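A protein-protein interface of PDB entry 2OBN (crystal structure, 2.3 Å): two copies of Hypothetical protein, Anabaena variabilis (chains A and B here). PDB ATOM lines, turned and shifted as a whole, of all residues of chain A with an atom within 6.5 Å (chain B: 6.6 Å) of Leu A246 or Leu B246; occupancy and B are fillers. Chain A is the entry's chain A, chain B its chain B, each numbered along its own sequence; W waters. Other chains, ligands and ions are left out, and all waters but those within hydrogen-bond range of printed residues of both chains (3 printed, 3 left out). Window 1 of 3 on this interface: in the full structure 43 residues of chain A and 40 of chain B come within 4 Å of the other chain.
Of the 15 printed residues of chain A, 7 touch a printed residue of chain B.
Of the 15 printed residues of chain B, 7 touch a printed residue of chain A.
Printed residues of chain B that touch a printed residue of chain A: Leu B237, Ser B242, Thr B243, Leu B246, Pro B247, Arg B250 and Val B289.
Among the printed residues, 13 pairs touch across the chains.
The backbone carbonyl oxygen of Leu A237 sits at hydrogen-bond distance from the guanidinium group of Arg B250 (2.9 Å).
NH2 of Arg A250 is in hydrogen-bond range of O of Leu B237 (2.9 Å).
Leu A246 touches four residues of chain B.
Leu B246 touches just these residues of chain A: Leu A237 (3.7 Å), Ser A242 (3.98 Å), Thr A243 (3.6 Å) and Leu A246 (3.8 Å).
Printed residues of chain A within 4 Å of Val B289: Val A289.
Printed residues of chain B within 4 Å of Leu A237: Leu B246 (3.7 Å) and Arg B250 (2.9 Å).
Leu A248 touches none of the printed residues of chain B.
The nearest residue of chain B that does not touch Leu A246 is Ala B244 (5.3 Å).
The nearest printed residue of chain A that does not touch Arg B250 is Ser A242 (4.3 Å).
Leu A237 touches Leu B246 (CD2 to CD2, 3.7 Å).
O of Ser A242 touches CD2 of Leu B246, 3.98 Å away.
Thr A243 touches Thr B243.
Thr A243 touches Leu B246 (O to CD2, 3.6 Å).
Thr A243 touches Pro B247 (OG1 to CB, 3.7 Å).
Leu A246 touches Ser B242.
CD2 of Leu A246 touches O of Thr B243 (3.5 Å).
CB of Leu A246 touches CD2 of Leu B246, 3.8 Å away.
OG1 of Thr B243 touches CB of Pro A247 (3.6 Å).
Val B289 touches Val A289.
Ser A242 touches Leu B246, and with the chains exchanged Leu A246 touches Ser B242.
Thr A243 touches Leu B246, and with the chains exchanged Leu A246 touches Thr B243.
Thr A243 touches Pro B247, and with the chains exchanged Pro A247 touches Thr B243.
Val B289 touches its own counterpart, Val A289.
Of the 13 pairs that touch across the chains among the printed residues, 13 have their exchanged pair printed and touching as well.
The side-chain hydroxyl (OG) of Ser A242 sits at hydrogen-bond distance from the backbone NH (N) of Ser A236, at 3.1 Å.
The guanidinium group of Arg A250 is in hydrogen-bond range of the backbone carbonyl oxygen of Val A289, at 3.0 Å.
N of Ser B236 is in hydrogen-bond range of OG of Ser B242 (3.2 Å).
O of Val B289 lies within hydrogen-bond range of NH1 of Arg B250 (3.0 Å).
Water W1 lies within hydrogen-bond range of the side-chain hydroxyl of Thr A243 (2.6 Å) and the backbone NH of Ala B212 (3.0 Å).
Water W3 bridges the side-chain hydroxyl of Thr B243 and the backbone NH of Ala A212.
Water W2 lies within hydrogen-bond range of O of Ser B242, NE of Arg A250 and O of Ser B236.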
ATOM      1  N   ALA A 212     -23.972  21.569 -13.733  1.00  0.00           N
ATOM      2  CA  ALA A 212     -23.554  20.639 -12.691  1.00  0.00           C
ATOM      3  C   ALA A 212     -24.769  19.892 -12.127  1.00  0.00           C
ATOM      4  O   ALA A 212     -24.717  18.667 -11.910  1.00  0.00           O
ATOM      5  CB  ALA A 212     -22.812  21.358 -11.599  1.00  0.00           C
ATOM      6  N   GLN A 234     -17.153  14.383 -21.845  1.00  0.00           N
ATOM      7  CA  GLN A 234     -17.403  15.406 -22.863  1.00  0.00           C
ATOM      8  C   GLN A 234     -16.297  16.424 -22.787  1.00  0.00           C
ATOM      9  O   GLN A 234     -15.739  16.698 -21.713  1.00  0.00           O
ATOM     10  CB  GLN A 234     -18.746  16.146 -22.667  1.00  0.00           C
ATOM     11  CG  GLN A 234     -19.986  15.260 -22.700  1.00  0.00           C
ATOM     12  CD  GLN A 234     -20.252  14.598 -24.044  1.00  0.00           C
ATOM     13  OE1 GLN A 234     -19.750  15.028 -25.084  1.00  0.00           O
ATOM     14  NE2 GLN A 234     -21.050  13.540 -24.023  1.00  0.00           N
ATOM     15  N   SER A 236     -12.851  18.691 -23.280  1.00  0.00           N
ATOM     16  CA  SER A 236     -11.482  18.532 -22.839  1.00  0.00           C
ATOM     17  C   SER A 236     -11.019  19.835 -22.251  1.00  0.00           C
ATOM     18  O   SER A 236     -11.269  20.884 -22.816  1.00  0.00           O
ATOM     19  CB  SER A 236     -10.556  18.170 -24.003  1.00  0.00           C
ATOM     20  OG  SER A 236      -9.209  18.229 -23.579  1.00  0.00           O
ATOM     21  N   LEU A 237     -10.323  19.770 -21.120  1.00  0.00           N
ATOM     22  CA  LEU A 237      -9.745  20.971 -20.522  1.00  0.00           C
ATOM     23  C   LEU A 237      -8.615  21.567 -21.371  1.00  0.00           C
ATOM     24  O   LEU A 237      -8.208  22.683 -21.134  1.00  0.00           O
ATOM     25  CB  LEU A 237      -9.270  20.679 -19.107  1.00  0.00           C
ATOM     26  CG  LEU A 237     -10.410  20.323 -18.148  1.00  0.00           C
ATOM     27  CD1 LEU A 237      -9.840  19.956 -16.780  1.00  0.00           C
ATOM     28  CD2 LEU A 237     -11.416  21.468 -18.030  1.00  0.00           C
ATOM     29  N   SER A 242     -13.976  24.487 -24.936  1.00  0.00           N
ATOM     30  CA  SER A 242     -14.717  23.493 -24.174  1.00  0.00           C
ATOM     31  C   SER A 242     -14.990  23.865 -22.714  1.00  0.00           C
ATOM     32  O   SER A 242     -14.092  24.315 -21.991  1.00  0.00           O
ATOM     33  CB  SER A 242     -13.967  22.159 -24.243  1.00  0.00           C
ATOM     34  OG  SER A 242     -14.669  21.165 -23.541  1.00  0.00           O
ATOM     35  N   THR A 243     -16.243  23.650 -22.309  1.00  0.00           N
ATOM     36  CA  THR A 243     -16.738  23.891 -20.947  1.00  0.00           C
ATOM     37  C   THR A 243     -17.212  22.629 -20.210  1.00  0.00           C
ATOM     38  O   THR A 243     -17.024  22.505 -18.994  1.00  0.00           O
ATOM     39  CB  THR A 243     -17.917  24.876 -21.017  1.00  0.00           C
ATOM     40  OG1 THR A 243     -17.429  26.158 -21.419  1.00  0.00           O
ATOM     41  CG2 THR A 243     -18.620  25.024 -19.687  1.00  0.00           C
ATOM     42  N   ALA A 244     -17.800  21.692 -20.946  1.00  0.00           N
ATOM     43  CA  ALA A 244     -18.467  20.514 -20.377  1.00  0.00           C
ATOM     44  C   ALA A 244     -17.741  19.655 -19.361  1.00  0.00           C
ATOM     45  O   ALA A 244     -18.393  19.088 -18.473  1.00  0.00           O
ATOM     46  CB  ALA A 244     -18.998  19.624 -21.487  1.00  0.00           C
ATOM     47  N   THR A 245     -16.423  19.556 -19.439  1.00  0.00           N
ATOM     48  CA  THR A 245     -15.741  18.656 -18.515  1.00  0.00           C
ATOM     49  C   THR A 245     -15.921  19.029 -17.036  1.00  0.00           C
ATOM     50  O   THR A 245     -16.011  18.138 -16.186  1.00  0.00           O
ATOM     51  CB  THR A 245     -14.243  18.491 -18.868  1.00  0.00           C
ATOM     52  OG1 THR A 245     -14.105  18.235 -20.273  1.00  0.00           O
ATOM     53  CG2 THR A 245     -13.636  17.334 -18.088  1.00  0.00           C
ATOM     54  N   LEU A 246     -16.011  20.327 -16.739  1.00  0.00           N
ATOM     55  CA  LEU A 246     -16.139  20.806 -15.360  1.00  0.00           C
ATOM     56  C   LEU A 246     -17.454  20.406 -14.698  1.00  0.00           C
ATOM     57  O   LEU A 246     -17.436  19.862 -13.576  1.00  0.00           O
ATOM     58  CB  LEU A 246     -15.947  22.332 -15.291  1.00  0.00           C
ATOM     59  CG  LEU A 246     -16.017  23.007 -13.921  1.00  0.00           C
ATOM     60  CD1 LEU A 246     -14.982  22.382 -12.977  1.00  0.00           C
ATOM     61  CD2 LEU A 246     -15.818  24.519 -14.039  1.00  0.00           C
ATOM     62  N   PRO A 247     -18.596  20.766 -15.321  1.00  0.00           N
ATOM     63  CA  PRO A 247     -19.840  20.295 -14.734  1.00  0.00           C
ATOM     64  C   PRO A 247     -19.919  18.781 -14.604  1.00  0.00           C
ATOM     65  O   PRO A 247     -20.535  18.307 -13.654  1.00  0.00           O
ATOM     66  CB  PRO A 247     -20.926  20.859 -15.661  1.00  0.00           C
ATOM     67  CG  PRO A 247     -20.225  21.312 -16.883  1.00  0.00           C
ATOM     68  CD  PRO A 247     -18.846  21.665 -16.460  1.00  0.00           C
ATOM     69  N   LEU A 248     -19.294  18.026 -15.510  1.00  0.00           N
ATOM     70  CA  LEU A 248     -19.282  16.559 -15.363  1.00  0.00           C
ATOM     71  C   LEU A 248     -18.559  16.154 -14.085  1.00  0.00           C
ATOM     72  O   LEU A 248     -19.049  15.326 -13.326  1.00  0.00           O
ATOM     73  CB  LEU A 248     -18.649  15.855 -16.567  1.00  0.00           C
ATOM     74  CG  LEU A 248     -19.478  15.845 -17.852  1.00  0.00           C
ATOM     75  CD1 LEU A 248     -18.610  15.397 -19.015  1.00  0.00           C
ATOM     76  CD2 LEU A 248     -20.715  14.969 -17.711  1.00  0.00           C
ATOM     77  N   ILE A 249     -17.396  16.743 -13.856  1.00  0.00           N
ATOM     78  CA  ILE A 249     -16.630  16.462 -12.651  1.00  0.00           C
ATOM     79  C   ILE A 249     -17.419  16.948 -11.414  1.00  0.00           C
ATOM     80  O   ILE A 249     -17.631  16.202 -10.457  1.00  0.00           O
ATOM     81  CB  ILE A 249     -15.205  17.111 -12.728  1.00  0.00           C
ATOM     82  CG1 ILE A 249     -14.352  16.405 -13.779  1.00  0.00           C
ATOM     83  CG2 ILE A 249     -14.481  17.022 -11.392  1.00  0.00           C
ATOM     84  CD1 ILE A 249     -13.015  17.125 -14.095  1.00  0.00           C
ATOM     85  N   ARG A 250     -17.888  18.182 -11.446  1.00  0.00           N
ATOM     86  CA  ARG A 250     -18.584  18.727 -10.281  1.00  0.00           C
ATOM     87  C   ARG A 250     -19.860  18.000  -9.904  1.00  0.00           C
ATOM     88  O   ARG A 250     -20.055  17.705  -8.717  1.00  0.00           O
ATOM     89  CB  ARG A 250     -18.854  20.221 -10.453  1.00  0.00           C
ATOM     90  CG  ARG A 250     -17.601  21.084 -10.419  1.00  0.00           C
ATOM     91  CD  ARG A 250     -17.033  21.252  -9.006  1.00  0.00           C
ATOM     92  NE  ARG A 250     -15.763  21.974  -9.076  1.00  0.00           N
ATOM     93  CZ  ARG A 250     -14.573  21.408  -9.302  1.00  0.00           C
ATOM     94  NH1 ARG A 250     -14.434  20.084  -9.406  1.00  0.00           N
ATOM     95  NH2 ARG A 250     -13.499  22.183  -9.359  1.00  0.00           N
ATOM     96  N   GLY A 251     -20.718  17.729 -10.892  1.00  0.00           N
ATOM     97  CA  GLY A 251     -21.993  17.052 -10.669  1.00  0.00           C
ATOM     98  C   GLY A 251     -21.930  15.583 -10.282  1.00  0.00           C
ATOM     99  O   GLY A 251     -22.756  15.089  -9.508  1.00  0.00           O
ATOM    100  N   VAL A 289      -8.206  19.804 -10.834  1.00  0.00           N
ATOM    101  CA  VAL A 289      -9.579  20.286 -11.030  1.00  0.00           C
ATOM    102  C   VAL A 289     -10.558  19.418 -10.250  1.00  0.00           C
ATOM    103  O   VAL A 289     -11.441  19.954  -9.592  1.00  0.00           O
ATOM    104  CB  VAL A 289      -9.977  20.352 -12.510  1.00  0.00           C
ATOM    105  CG1 VAL A 289     -11.480  20.527 -12.682  1.00  0.00           C
ATOM    106  CG2 VAL A 289      -9.234  21.475 -13.182  1.00  0.00           C
ATOM    107  N   ALA B 212     -18.077  29.633 -23.738  1.00  0.00           N
ATOM    108  CA  ALA B 212     -16.768  30.206 -24.020  1.00  0.00           C
ATOM    109  C   ALA B 212     -16.860  31.173 -25.194  1.00  0.00           C
ATOM    110  O   ALA B 212     -16.209  32.223 -25.199  1.00  0.00           O
ATOM    111  CB  ALA B 212     -15.757  29.096 -24.314  1.00  0.00           C
ATOM    112  N   GLN B 234     -17.245  35.322 -12.394  1.00  0.00           N
ATOM    113  CA  GLN B 234     -18.463  34.620 -11.992  1.00  0.00           C
ATOM    114  C   GLN B 234     -18.082  33.237 -11.471  1.00  0.00           C
ATOM    115  O   GLN B 234     -17.131  32.609 -11.953  1.00  0.00           O
ATOM    116  CB  GLN B 234     -19.448  34.448 -13.148  1.00  0.00           C
ATOM    117  CG  GLN B 234     -19.873  35.701 -13.888  1.00  0.00           C
ATOM    118  CD  GLN B 234     -20.783  36.617 -13.089  1.00  0.00           C
ATOM    119  OE1 GLN B 234     -21.321  36.235 -12.041  1.00  0.00           O
ATOM    120  NE2 GLN B 234     -20.990  37.831 -13.607  1.00  0.00           N
ATOM    121  N   SER B 236     -16.973  30.012  -8.968  1.00  0.00           N
ATOM    122  CA  SER B 236     -15.765  29.631  -8.269  1.00  0.00           C
ATOM    123  C   SER B 236     -15.465  28.173  -8.525  1.00  0.00           C
ATOM    124  O   SER B 236     -16.373  27.337  -8.489  1.00  0.00           O
ATOM    125  CB  SER B 236     -15.930  29.795  -6.757  1.00  0.00           C
ATOM    126  OG  SER B 236     -14.788  29.270  -6.090  1.00  0.00           O
ATOM    127  N   LEU B 237     -14.189  27.849  -8.713  1.00  0.00           N
ATOM    128  CA  LEU B 237     -13.792  26.458  -8.882  1.00  0.00           C
ATOM    129  C   LEU B 237     -13.898  25.666  -7.569  1.00  0.00           C
ATOM    130  O   LEU B 237     -13.628  24.475  -7.563  1.00  0.00           O
ATOM    131  CB  LEU B 237     -12.363  26.372  -9.444  1.00  0.00           C
ATOM    132  CG  LEU B 237     -12.145  26.915 -10.861  1.00  0.00           C
ATOM    133  CD1 LEU B 237     -10.671  26.818 -11.209  1.00  0.00           C
ATOM    134  CD2 LEU B 237     -12.981  26.177 -11.881  1.00  0.00           C
ATOM    135  N   SER B 242     -20.886  25.321  -9.518  1.00  0.00           N
ATOM    136  CA  SER B 242     -20.452  26.356 -10.431  1.00  0.00           C
ATOM    137  C   SER B 242     -19.627  25.857 -11.608  1.00  0.00           C
ATOM    138  O   SER B 242     -18.760  24.984 -11.475  1.00  0.00           O
ATOM    139  CB  SER B 242     -19.624  27.380  -9.665  1.00  0.00           C
ATOM    140  OG  SER B 242     -19.207  28.426 -10.525  1.00  0.00           O
ATOM    141  N   THR B 243     -19.898  26.466 -12.757  1.00  0.00           N
ATOM    142  CA  THR B 243     -19.252  26.154 -14.028  1.00  0.00           C
ATOM    143  C   THR B 243     -18.619  27.369 -14.688  1.00  0.00           C
ATOM    144  O   THR B 243     -17.616  27.235 -15.378  1.00  0.00           O
ATOM    145  CB  THR B 243     -20.339  25.589 -15.020  1.00  0.00           C
ATOM    146  OG1 THR B 243     -20.793  24.304 -14.583  1.00  0.00           O
ATOM    147  CG2 THR B 243     -19.852  25.465 -16.439  1.00  0.00           C
ATOM    148  N   ALA B 244     -19.196  28.551 -14.466  1.00  0.00           N
ATOM    149  CA  ALA B 244     -18.880  29.747 -15.266  1.00  0.00           C
ATOM    150  C   ALA B 244     -17.448  30.243 -15.305  1.00  0.00           C
ATOM    151  O   ALA B 244     -17.075  30.983 -16.215  1.00  0.00           O
ATOM    152  CB  ALA B 244     -19.807  30.897 -14.864  1.00  0.00           C
ATOM    153  N   THR B 245     -16.643  29.875 -14.326  1.00  0.00           N
ATOM    154  CA  THR B 245     -15.259  30.307 -14.339  1.00  0.00           C
ATOM    155  C   THR B 245     -14.499  29.725 -15.537  1.00  0.00           C
ATOM    156  O   THR B 245     -13.660  30.414 -16.116  1.00  0.00           O
ATOM    157  CB  THR B 245     -14.508  29.901 -13.049  1.00  0.00           C
ATOM    158  OG1 THR B 245     -15.225  30.358 -11.899  1.00  0.00           O
ATOM    159  CG2 THR B 245     -13.123  30.526 -13.043  1.00  0.00           C
ATOM    160  N   LEU B 246     -14.788  28.481 -15.916  1.00  0.00           N
ATOM    161  CA  LEU B 246     -14.030  27.860 -17.000  1.00  0.00           C
ATOM    162  C   LEU B 246     -14.192  28.617 -18.341  1.00  0.00           C
ATOM    163  O   LEU B 246     -13.182  29.005 -18.936  1.00  0.00           O
ATOM    164  CB  LEU B 246     -14.334  26.367 -17.107  1.00  0.00           C
ATOM    165  CG  LEU B 246     -13.554  25.551 -18.135  1.00  0.00           C
ATOM    166  CD1 LEU B 246     -12.023  25.716 -18.001  1.00  0.00           C
ATOM    167  CD2 LEU B 246     -13.983  24.079 -18.020  1.00  0.00           C
ATOM    168  N   PRO B 247     -15.446  28.829 -18.820  1.00  0.00           N
ATOM    169  CA  PRO B 247     -15.598  29.634 -20.047  1.00  0.00           C
ATOM    170  C   PRO B 247     -15.061  31.062 -19.944  1.00  0.00           C
ATOM    171  O   PRO B 247     -14.616  31.607 -20.944  1.00  0.00           O
ATOM    172  CB  PRO B 247     -17.117  29.633 -20.296  1.00  0.00           C
ATOM    173  CG  PRO B 247     -17.742  29.176 -19.000  1.00  0.00           C
ATOM    174  CD  PRO B 247     -16.742  28.291 -18.359  1.00  0.00           C
ATOM    175  N   LEU B 248     -15.111  31.681 -18.768  1.00  0.00           N
ATOM    176  CA  LEU B 248     -14.524  33.029 -18.615  1.00  0.00           C
ATOM    177  C   LEU B 248     -13.033  33.002 -18.941  1.00  0.00           C
ATOM    178  O   LEU B 248     -12.548  33.815 -19.723  1.00  0.00           O
ATOM    179  CB  LEU B 248     -14.763  33.581 -17.214  1.00  0.00           C
ATOM    180  CG  LEU B 248     -16.208  34.027 -16.981  1.00  0.00           C
ATOM    181  CD1 LEU B 248     -16.469  34.319 -15.510  1.00  0.00           C
ATOM    182  CD2 LEU B 248     -16.551  35.230 -17.822  1.00  0.00           C
ATOM    183  N   ILE B 249     -12.331  32.033 -18.364  1.00  0.00           N
ATOM    184  CA  ILE B 249     -10.900  31.841 -18.602  1.00  0.00           C
ATOM    185  C   ILE B 249     -10.597  31.452 -20.066  1.00  0.00           C
ATOM    186  O   ILE B 249      -9.702  31.999 -20.691  1.00  0.00           O
ATOM    187  CB  ILE B 249     -10.332  30.766 -17.649  1.00  0.00           C
ATOM    188  CG1 ILE B 249     -10.312  31.301 -16.222  1.00  0.00           C
ATOM    189  CG2 ILE B 249      -8.921  30.356 -18.065  1.00  0.00           C
ATOM    190  CD1 ILE B 249      -9.867  30.287 -15.149  1.00  0.00           C
ATOM    191  N   ARG B 250     -11.339  30.491 -20.596  1.00  0.00           N
ATOM    192  CA  ARG B 250     -11.104  30.010 -21.951  1.00  0.00           C
ATOM    193  C   ARG B 250     -11.491  31.059 -22.981  1.00  0.00           C
ATOM    194  O   ARG B 250     -10.744  31.318 -23.939  1.00  0.00           O
ATOM    195  CB  ARG B 250     -11.878  28.710 -22.181  1.00  0.00           C
ATOM    196  CG  ARG B 250     -11.397  27.541 -21.332  1.00  0.00           C
ATOM    197  CD  ARG B 250     -10.136  26.887 -21.919  1.00  0.00           C
ATOM    198  NE  ARG B 250      -9.654  25.796 -21.073  1.00  0.00           N
ATOM    199  CZ  ARG B 250      -8.880  25.955 -20.005  1.00  0.00           C
ATOM    200  NH1 ARG B 250      -8.424  27.158 -19.654  1.00  0.00           N
ATOM    201  NH2 ARG B 250      -8.532  24.888 -19.298  1.00  0.00           N
ATOM    202  N   GLY B 251     -12.657  31.664 -22.807  1.00  0.00           N
ATOM    203  CA  GLY B 251     -13.107  32.684 -23.755  1.00  0.00           C
ATOM    204  C   GLY B 251     -12.261  33.949 -23.777  1.00  0.00           C
ATOM    205  O   GLY B 251     -11.982  34.475 -24.840  1.00  0.00           O
ATOM    206  N   VAL B 289      -5.485  25.565 -14.206  1.00  0.00           N
ATOM    207  CA  VAL B 289      -6.651  25.626 -15.101  1.00  0.00           C
ATOM    208  C   VAL B 289      -6.396  26.636 -16.216  1.00  0.00           C
ATOM    209  O   VAL B 289      -6.640  26.347 -17.378  1.00  0.00           O
ATOM    210  CB  VAL B 289      -7.969  25.984 -14.346  1.00  0.00           C
ATOM    211  CG1 VAL B 289      -9.140  26.251 -15.309  1.00  0.00           C
ATOM    212  CG2 VAL B 289      -8.365  24.857 -13.399  1.00  0.00           C
HETATM  213  O   HOH W   1     -18.093  26.650 -23.840  1.00  0.00           O
HETATM  214  O   HOH W   2     -16.671  24.620  -9.718  1.00  0.00           O
HETATM  215  O   HOH W   3     -23.015  24.476 -13.251  1.00  0.00           O
